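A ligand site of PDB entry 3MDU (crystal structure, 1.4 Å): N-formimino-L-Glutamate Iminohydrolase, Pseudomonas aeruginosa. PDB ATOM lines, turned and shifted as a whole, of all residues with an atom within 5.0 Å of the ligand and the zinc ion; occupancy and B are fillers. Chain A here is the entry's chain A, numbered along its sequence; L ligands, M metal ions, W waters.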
ATOM      1  N   HIS A  56      10.259  32.767 -27.146  1.00  0.00           N
ATOM      2  CA  HIS A  56      11.375  32.013 -26.594  1.00  0.00           C
ATOM      3  C   HIS A  56      12.662  32.233 -27.373  1.00  0.00           C
ATOM      4  O   HIS A  56      12.732  31.938 -28.563  1.00  0.00           O
ATOM      5  CB  HIS A  56      11.027  30.530 -26.592  1.00  0.00           C
ATOM      6  CG  HIS A  56      12.027  29.669 -25.883  1.00  0.00           C
ATOM      7  ND1 HIS A  56      12.160  29.663 -24.516  1.00  0.00           N
ATOM      8  CD2 HIS A  56      12.922  28.776 -26.361  1.00  0.00           C
ATOM      9  CE1 HIS A  56      13.108  28.799 -24.175  1.00  0.00           C
ATOM     10  NE2 HIS A  56      13.581  28.246 -25.273  1.00  0.00           N
ATOM     11  N   HIS A  58      17.247  32.268 -26.896  1.00  0.00           N
ATOM     12  CA  HIS A  58      18.532  32.348 -26.177  1.00  0.00           C
ATOM     13  C   HIS A  58      19.483  33.079 -27.119  1.00  0.00           C
ATOM     14  O   HIS A  58      20.056  32.473 -28.017  1.00  0.00           O
ATOM     15  CB  HIS A  58      19.112  30.973 -25.830  1.00  0.00           C
ATOM     16  CG  HIS A  58      18.102  30.021 -25.281  1.00  0.00           C
ATOM     17  ND1 HIS A  58      17.410  30.245 -24.108  1.00  0.00           N
ATOM     18  CD2 HIS A  58      17.659  28.828 -25.753  1.00  0.00           C
ATOM     19  CE1 HIS A  58      16.578  29.251 -23.884  1.00  0.00           C
ATOM     20  NE2 HIS A  58      16.703  28.376 -24.869  1.00  0.00           N
ATOM     21  N   GLN A  61      22.926  32.089 -28.924  1.00  0.00           N
ATOM     22  CA  GLN A  61      22.987  30.943 -29.825  1.00  0.00           C
ATOM     23  C   GLN A  61      22.984  31.337 -31.297  1.00  0.00           C
ATOM     24  O   GLN A  61      23.435  30.573 -32.150  1.00  0.00           O
ATOM     25  CB  GLN A  61      21.888  29.923 -29.493  1.00  0.00           C
ATOM     26  CG  GLN A  61      22.151  29.260 -28.123  1.00  0.00           C
ATOM     27  CD  GLN A  61      21.115  28.225 -27.723  1.00  0.00           C
ATOM     28  OE1 GLN A  61      20.303  27.770 -28.546  1.00  0.00           O
ATOM     29  NE2 GLN A  61      21.125  27.844 -26.445  1.00  0.00           N
ATOM     30  N   PHE A  78      20.600  15.926 -29.901  1.00  0.00           N
ATOM     31  CA  PHE A  78      20.498  17.104 -29.064  1.00  0.00           C
ATOM     32  C   PHE A  78      21.629  17.168 -28.036  1.00  0.00           C
ATOM     33  O   PHE A  78      22.134  18.253 -27.715  1.00  0.00           O
ATOM     34  CB  PHE A  78      19.133  17.077 -28.361  1.00  0.00           C
ATOM     35  CG  PHE A  78      19.020  18.067 -27.241  1.00  0.00           C
ATOM     36  CD1 PHE A  78      18.490  19.329 -27.471  1.00  0.00           C
ATOM     37  CD2 PHE A  78      19.433  17.733 -25.970  1.00  0.00           C
ATOM     38  CE1 PHE A  78      18.388  20.239 -26.434  1.00  0.00           C
ATOM     39  CE2 PHE A  78      19.329  18.634 -24.929  1.00  0.00           C
ATOM     40  CZ  PHE A  78      18.812  19.892 -25.160  1.00  0.00           C
ATOM     41  N   TRP A  81      25.004  18.127 -29.545  1.00  0.00           N
ATOM     42  CA  TRP A  81      24.836  19.541 -29.859  1.00  0.00           C
ATOM     43  C   TRP A  81      25.053  20.405 -28.615  1.00  0.00           C
ATOM     44  O   TRP A  81      25.690  21.466 -28.692  1.00  0.00           O
ATOM     45  CB  TRP A  81      23.450  19.797 -30.439  1.00  0.00           C
ATOM     46  CG  TRP A  81      23.095  21.242 -30.551  1.00  0.00           C
ATOM     47  CD1 TRP A  81      23.358  22.072 -31.605  1.00  0.00           C
ATOM     48  CD2 TRP A  81      22.417  22.051 -29.576  1.00  0.00           C
ATOM     49  NE1 TRP A  81      22.875  23.330 -31.343  1.00  0.00           N
ATOM     50  CE2 TRP A  81      22.286  23.348 -30.109  1.00  0.00           C
ATOM     51  CE3 TRP A  81      21.883  21.791 -28.302  1.00  0.00           C
ATOM     52  CZ2 TRP A  81      21.683  24.382 -29.419  1.00  0.00           C
ATOM     53  CZ3 TRP A  81      21.275  22.835 -27.620  1.00  0.00           C
ATOM     54  CH2 TRP A  81      21.173  24.115 -28.177  1.00  0.00           C
ATOM     55  N   ARG A  82      24.515  19.946 -27.488  1.00  0.00           N
ATOM     56  CA  ARG A  82      24.576  20.720 -26.251  1.00  0.00           C
ATOM     57  C   ARG A  82      26.011  20.959 -25.818  1.00  0.00           C
ATOM     58  O   ARG A  82      26.334  22.020 -25.287  1.00  0.00           O
ATOM     59  CB  ARG A  82      23.774  20.054 -25.141  1.00  0.00           C
ATOM     60  CG  ARG A  82      23.583  20.952 -23.915  1.00  0.00           C
ATOM     61  CD  ARG A  82      22.722  20.300 -22.842  1.00  0.00           C
ATOM     62  NE  ARG A  82      23.472  19.351 -22.031  1.00  0.00           N
ATOM     63  CZ  ARG A  82      23.092  18.919 -20.832  1.00  0.00           C
ATOM     64  NH1 ARG A  82      21.955  19.349 -20.299  1.00  0.00           N
ATOM     65  NH2 ARG A  82      23.846  18.053 -20.177  1.00  0.00           N
ATOM     66  N   MET A  85      27.364  23.831 -27.788  1.00  0.00           N
ATOM     67  CA  MET A  85      26.796  25.070 -27.261  1.00  0.00           C
ATOM     68  C   MET A  85      27.530  25.490 -25.979  1.00  0.00           C
ATOM     69  O   MET A  85      27.862  26.660 -25.795  1.00  0.00           O
ATOM     70  CB  MET A  85      25.298  24.899 -27.037  1.00  0.00           C
ATOM     71  CG  MET A  85      24.549  26.157 -26.600  1.00  0.00           C
ATOM     72  SD  MET A  85      24.548  26.370 -24.815  1.00  0.00           S
ATOM     73  CE  MET A  85      23.237  25.247 -24.331  1.00  0.00           C
ATOM     74  N   TYR A  86      27.785  24.518 -25.106  1.00  0.00           N
ATOM     75  CA  TYR A  86      28.547  24.787 -23.880  1.00  0.00           C
ATOM     76  C   TYR A  86      29.940  25.352 -24.194  1.00  0.00           C
ATOM     77  O   TYR A  86      30.423  26.259 -23.509  1.00  0.00           O
ATOM     78  CB  TYR A  86      28.692  23.511 -23.046  1.00  0.00           C
ATOM     79  CG  TYR A  86      27.468  23.112 -22.252  1.00  0.00           C
ATOM     80  CD1 TYR A  86      26.287  23.856 -22.297  1.00  0.00           C
ATOM     81  CD2 TYR A  86      27.482  21.970 -21.457  1.00  0.00           C
ATOM     82  CE1 TYR A  86      25.167  23.473 -21.560  1.00  0.00           C
ATOM     83  CE2 TYR A  86      26.383  21.587 -20.732  1.00  0.00           C
ATOM     84  CZ  TYR A  86      25.226  22.336 -20.775  1.00  0.00           C
ATOM     85  OH  TYR A  86      24.146  21.935 -20.025  1.00  0.00           O
ATOM     86  N   TYR A 121      19.886  32.556 -19.294  1.00  0.00           N
ATOM     87  CA  TYR A 121      20.550  31.777 -18.249  1.00  0.00           C
ATOM     88  C   TYR A 121      22.064  31.983 -18.192  1.00  0.00           C
ATOM     89  O   TYR A 121      22.734  31.341 -17.388  1.00  0.00           O
ATOM     90  CB  TYR A 121      20.239  30.292 -18.397  1.00  0.00           C
ATOM     91  CG  TYR A 121      20.523  29.729 -19.779  1.00  0.00           C
ATOM     92  CD1 TYR A 121      21.820  29.504 -20.206  1.00  0.00           C
ATOM     93  CD2 TYR A 121      19.488  29.403 -20.636  1.00  0.00           C
ATOM     94  CE1 TYR A 121      22.086  28.988 -21.479  1.00  0.00           C
ATOM     95  CE2 TYR A 121      19.720  28.886 -21.879  1.00  0.00           C
ATOM     96  CZ  TYR A 121      21.027  28.670 -22.303  1.00  0.00           C
ATOM     97  OH  TYR A 121      21.256  28.149 -23.559  1.00  0.00           O
ATOM     98  N   TYR A 159      18.697  28.051 -12.635  1.00  0.00           N
ATOM     99  CA  TYR A 159      19.409  26.874 -13.121  1.00  0.00           C
ATOM    100  C   TYR A 159      20.335  26.484 -11.988  1.00  0.00           C
ATOM    101  O   TYR A 159      21.162  27.287 -11.552  1.00  0.00           O
ATOM    102  CB  TYR A 159      20.223  27.230 -14.369  1.00  0.00           C
ATOM    103  CG  TYR A 159      20.669  26.049 -15.185  1.00  0.00           C
ATOM    104  CD1 TYR A 159      20.312  25.933 -16.520  1.00  0.00           C
ATOM    105  CD2 TYR A 159      21.466  25.046 -14.624  1.00  0.00           C
ATOM    106  CE1 TYR A 159      20.734  24.845 -17.285  1.00  0.00           C
ATOM    107  CE2 TYR A 159      21.890  23.963 -15.376  1.00  0.00           C
ATOM    108  CZ  TYR A 159      21.510  23.859 -16.695  1.00  0.00           C
ATOM    109  OH  TYR A 159      21.920  22.780 -17.446  1.00  0.00           O
ATOM    110  N   HIS A 206      14.797  26.632 -15.682  1.00  0.00           N
ATOM    111  CA  HIS A 206      15.346  26.131 -16.934  1.00  0.00           C
ATOM    112  C   HIS A 206      14.591  24.910 -17.455  1.00  0.00           C
ATOM    113  O   HIS A 206      14.213  24.839 -18.626  1.00  0.00           O
ATOM    114  CB  HIS A 206      16.835  25.808 -16.831  1.00  0.00           C
ATOM    115  CG  HIS A 206      17.392  25.294 -18.111  1.00  0.00           C
ATOM    116  ND1 HIS A 206      17.387  23.954 -18.435  1.00  0.00           N
ATOM    117  CD2 HIS A 206      17.905  25.935 -19.185  1.00  0.00           C
ATOM    118  CE1 HIS A 206      17.902  23.791 -19.638  1.00  0.00           C
ATOM    119  NE2 HIS A 206      18.226  24.979 -20.116  1.00  0.00           N
ATOM    120  N   ARG A 209      14.996  19.157 -15.114  1.00  0.00           N
ATOM    121  CA  ARG A 209      16.316  18.580 -14.903  1.00  0.00           C
ATOM    122  C   ARG A 209      17.205  19.502 -14.078  1.00  0.00           C
ATOM    123  O   ARG A 209      18.069  19.037 -13.334  1.00  0.00           O
ATOM    124  CB  ARG A 209      17.013  18.310 -16.252  1.00  0.00           C
ATOM    125  CG  ARG A 209      16.295  17.320 -17.157  1.00  0.00           C
ATOM    126  CD  ARG A 209      16.913  17.306 -18.564  1.00  0.00           C
ATOM    127  NE  ARG A 209      16.328  18.307 -19.462  1.00  0.00           N
ATOM    128  CZ  ARG A 209      16.979  19.358 -19.963  1.00  0.00           C
ATOM    129  NH1 ARG A 209      18.257  19.563 -19.653  1.00  0.00           N
ATOM    130  NH2 ARG A 209      16.364  20.197 -20.788  1.00  0.00           N
ATOM    131  N   HIS A 232      11.369  25.023 -19.892  1.00  0.00           N
ATOM    132  CA  HIS A 232      11.487  24.037 -20.968  1.00  0.00           C
ATOM    133  C   HIS A 232      10.915  22.735 -20.426  1.00  0.00           C
ATOM    134  O   HIS A 232      11.285  22.319 -19.316  1.00  0.00           O
ATOM    135  CB  HIS A 232      12.955  23.686 -21.275  1.00  0.00           C
ATOM    136  CG  HIS A 232      13.763  24.751 -21.971  1.00  0.00           C
ATOM    137  ND1 HIS A 232      14.892  25.289 -21.390  1.00  0.00           N
ATOM    138  CD2 HIS A 232      13.697  25.270 -23.221  1.00  0.00           C
ATOM    139  CE1 HIS A 232      15.447  26.149 -22.233  1.00  0.00           C
ATOM    140  NE2 HIS A 232      14.759  26.143 -23.355  1.00  0.00           N
ATOM    141  N   GLU A 235      10.839  18.257 -24.048  1.00  0.00           N
ATOM    142  CA  GLU A 235      11.402  18.442 -25.380  1.00  0.00           C
ATOM    143  C   GLU A 235      11.913  17.160 -26.033  1.00  0.00           C
ATOM    144  O   GLU A 235      11.628  16.889 -27.196  1.00  0.00           O
ATOM    145  CB  GLU A 235      12.525  19.478 -25.359  1.00  0.00           C
ATOM    146  CG  GLU A 235      13.031  19.824 -26.746  1.00  0.00           C
ATOM    147  CD  GLU A 235      14.188  20.793 -26.702  1.00  0.00           C
ATOM    148  OE1 GLU A 235      14.638  21.129 -25.593  1.00  0.00           O
ATOM    149  OE2 GLU A 235      14.646  21.223 -27.788  1.00  0.00           O
ATOM    150  N   VAL A 268       7.576  25.532 -22.680  1.00  0.00           N
ATOM    151  CA  VAL A 268       8.344  25.583 -23.919  1.00  0.00           C
ATOM    152  C   VAL A 268       8.600  24.189 -24.447  1.00  0.00           C
ATOM    153  O   VAL A 268       9.042  23.302 -23.707  1.00  0.00           O
ATOM    154  CB  VAL A 268       9.684  26.340 -23.739  1.00  0.00           C
ATOM    155  CG1 VAL A 268      10.365  26.499 -25.079  1.00  0.00           C
ATOM    156  CG2 VAL A 268       9.434  27.700 -23.119  1.00  0.00           C
ATOM    157  N   HIS A 269       8.311  24.015 -25.739  1.00  0.00           N
ATOM    158  CA  HIS A 269       8.370  22.740 -26.453  1.00  0.00           C
ATOM    159  C   HIS A 269       7.164  21.854 -26.143  1.00  0.00           C
ATOM    160  O   HIS A 269       6.275  21.694 -26.977  1.00  0.00           O
ATOM    161  CB  HIS A 269       9.686  21.984 -26.221  1.00  0.00           C
ATOM    162  CG  HIS A 269      10.906  22.820 -26.450  1.00  0.00           C
ATOM    163  ND1 HIS A 269      11.165  23.452 -27.652  1.00  0.00           N
ATOM    164  CD2 HIS A 269      11.939  23.129 -25.640  1.00  0.00           C
ATOM    165  CE1 HIS A 269      12.305  24.107 -27.572  1.00  0.00           C
ATOM    166  NE2 HIS A 269      12.799  23.926 -26.359  1.00  0.00           N
ATOM    167  N   THR A 294      13.786  25.157 -34.475  1.00  0.00           N
ATOM    168  CA  THR A 294      14.779  24.601 -33.553  1.00  0.00           C
ATOM    169  C   THR A 294      14.464  23.139 -33.208  1.00  0.00           C
ATOM    170  O   THR A 294      15.376  22.303 -33.171  1.00  0.00           O
ATOM    171  CB  THR A 294      14.938  25.437 -32.281  1.00  0.00           C
ATOM    172  OG1 THR A 294      15.613  26.669 -32.609  1.00  0.00           O
ATOM    173  CG2 THR A 294      15.778  24.694 -31.237  1.00  0.00           C
ATOM    174  N   LEU A 298      17.005  20.190 -33.913  1.00  0.00           N
ATOM    175  CA  LEU A 298      17.516  19.363 -32.814  1.00  0.00           C
ATOM    176  C   LEU A 298      16.962  17.942 -32.834  1.00  0.00           C
ATOM    177  O   LEU A 298      17.355  17.111 -32.012  1.00  0.00           O
ATOM    178  CB  LEU A 298      17.241  20.039 -31.477  1.00  0.00           C
ATOM    179  CG  LEU A 298      17.965  21.377 -31.282  1.00  0.00           C
ATOM    180  CD1 LEU A 298      17.592  21.981 -29.948  1.00  0.00           C
ATOM    181  CD2 LEU A 298      19.476  21.233 -31.392  1.00  0.00           C
ATOM    182  N   ASP A 320      14.114  30.457 -30.480  1.00  0.00           N
ATOM    183  CA  ASP A 320      14.925  29.570 -29.634  1.00  0.00           C
ATOM    184  C   ASP A 320      16.450  29.603 -29.879  1.00  0.00           C
ATOM    185  O   ASP A 320      17.133  30.488 -29.364  1.00  0.00           O
ATOM    186  CB  ASP A 320      14.371  28.141 -29.705  1.00  0.00           C
ATOM    187  CG  ASP A 320      14.886  27.252 -28.593  1.00  0.00           C
ATOM    188  OD1 ASP A 320      15.589  27.731 -27.673  1.00  0.00           O
ATOM    189  OD2 ASP A 320      14.578  26.047 -28.643  1.00  0.00           O
HETATM  190  C1  LIG L   1      19.219  25.678 -23.705  1.00  0.00           C
HETATM  191  N1  LIG L   1      18.104  24.474 -25.504  1.00  0.00           N
HETATM  192  O1  LIG L   1      19.558  26.537 -24.541  1.00  0.00           O
HETATM  193  O2  LIG L   1      19.292  25.915 -22.472  1.00  0.00           O
HETATM  194  C2  LIG L   1      18.695  24.323 -24.169  1.00  0.00           C
HETATM  195  C3  LIG L   1      19.843  23.308 -24.251  1.00  0.00           C
HETATM  196  C4  LIG L   1      19.469  22.009 -22.093  1.00  0.00           C
HETATM  197  C5  LIG L   1      17.249  23.390 -25.973  1.00  0.00           C
HETATM  198  N2  LIG L   1      16.817  22.527 -25.161  1.00  0.00           N
HETATM  199  C6  LIG L   1      20.347  22.986 -22.850  1.00  0.00           C
HETATM  200  N3  LIG L   1      16.914  23.303 -27.186  1.00  0.00           N
HETATM  201  O3  LIG L   1      19.920  21.452 -21.060  1.00  0.00           O
HETATM  202  O4  LIG L   1      18.269  21.842 -22.423  1.00  0.00           O
HETATM  203 ZN    ZN M   1      15.231  27.000 -25.262  1.00  0.00          ZN
HETATM  204  O   HOH W   1      15.033  25.298 -26.188  1.00  0.00           O
HETATM  205  O   HOH W   2      18.090  26.075 -27.892  1.00  0.00           O
HETATM  206  O   HOH W   3      21.559  25.759 -20.931  1.00  0.00           O
HETATM  207  O   HOH W   4      14.534  21.233 -23.063  1.00  0.00           O
HETATM  208  O   HOH W   5      21.817  23.209 -20.127  1.00  0.00           O
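Within 4 Å of the zinc ion: His 56, His 58, His 232 and Asp 320. Along chain A the residues within 4 Å of the zinc ion span positions 56 to 320.
The zinc ion is bound by water W1 (1.9 Å), NE2 of His 58 (2.1 Å), NE2 of His 56 (2.1 Å), NE2 of His 232 (2.1 Å) and OD1 of Asp 320 (2.5 Å). The zinc ion has five donor atoms within binding distance.
A ring nitrogen (NE2) of His 58 lies close to an oxygen (O1) of the ligand, 3.4 Å away. OH of Tyr 121 lies within hydrogen-bond range of O1 of the ligand (2.5 Å). A nitrogen (N3) of the ligand lies within salt-bridge range of the side-chain carboxylate (OD2) of Asp 320, 3.9 Å away. The side-chain carboxylate of Glu 235 is in salt-bridge range of a nitrogen (N2) of the ligand (2.6 Å). An oxygen (O2) of the ligand sits at hydrogen-bond distance from a ring nitrogen (NE2) of His 206 (2.8 Å). NE2 of Gln 61 lies within hydrogen-bond range of O1 of the ligand (2.8 Å). O3 of the ligand is in salt-bridge range of NH1 of Arg 209 (2.9 Å). An oxygen (O3) of the ligand lies within salt-bridge range of the guanidinium group of Arg 82 (3.0 Å).
Phe 78 touches the ligand (CE1 to N2, 3.1 Å). Trp 81 touches the ligand (CZ3 to C3, 3.7 Å). Met 85 touches the ligand (CE to O1, 3.9 Å). Leu 298 touches the ligand. Hydrophobic or aromatic side chains within 4 Å of the ligand: His 58, Phe 78, Trp 81, Met 85, Tyr 121, His 206, His 232 and Leu 298. 13 residues have an atom within 4 Å of the ligand: His 58, Gln 61, Phe 78, Trp 81, Arg 82, Met 85, Tyr 121, His 206, Arg 209, His 232, Glu 235, Leu 298 and Asp 320.
Water W1 lies within hydrogen-bond range of the side-chain carboxylate of Asp 320 (2.6 Å), a ring nitrogen (NE2) of His 269 (2.6 Å) and a nitrogen (N3) of the ligand (2.9 Å). Water W5 lies within hydrogen-bond range of the side-chain hydroxyl (OH) of Tyr 86 (2.7 Å), the side-chain hydroxyl (OH) of Tyr 159 (2.7 Å) and an oxygen (O3) of the ligand (2.7 Å). Water W2 bridges the side-chain amide oxygen of Gln 61 (2.9 Å) and a nitrogen (N1) of the ligand (2.9 Å). Water W4 lies within hydrogen-bond range of the side-chain carboxylate (OE1) of Glu 235, the guanidinium group (NH2) of Arg 209 and a nitrogen (N2) of the ligand.
O of His 206 is in hydrogen-bond range of ND1 of His 232 (2.9 Å). The side-chain amide nitrogen of Gln 61 is in hydrogen-bond range of the side-chain hydroxyl of Tyr 121 (2.9 Å). A ring nitrogen (NE2) of His 269 sits close to the side-chain carboxylate of Glu 235 (3.4 Å). The side-chain hydroxyl of Tyr 86 lies close to the guanidinium group of Arg 82, 3.3 Å away.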
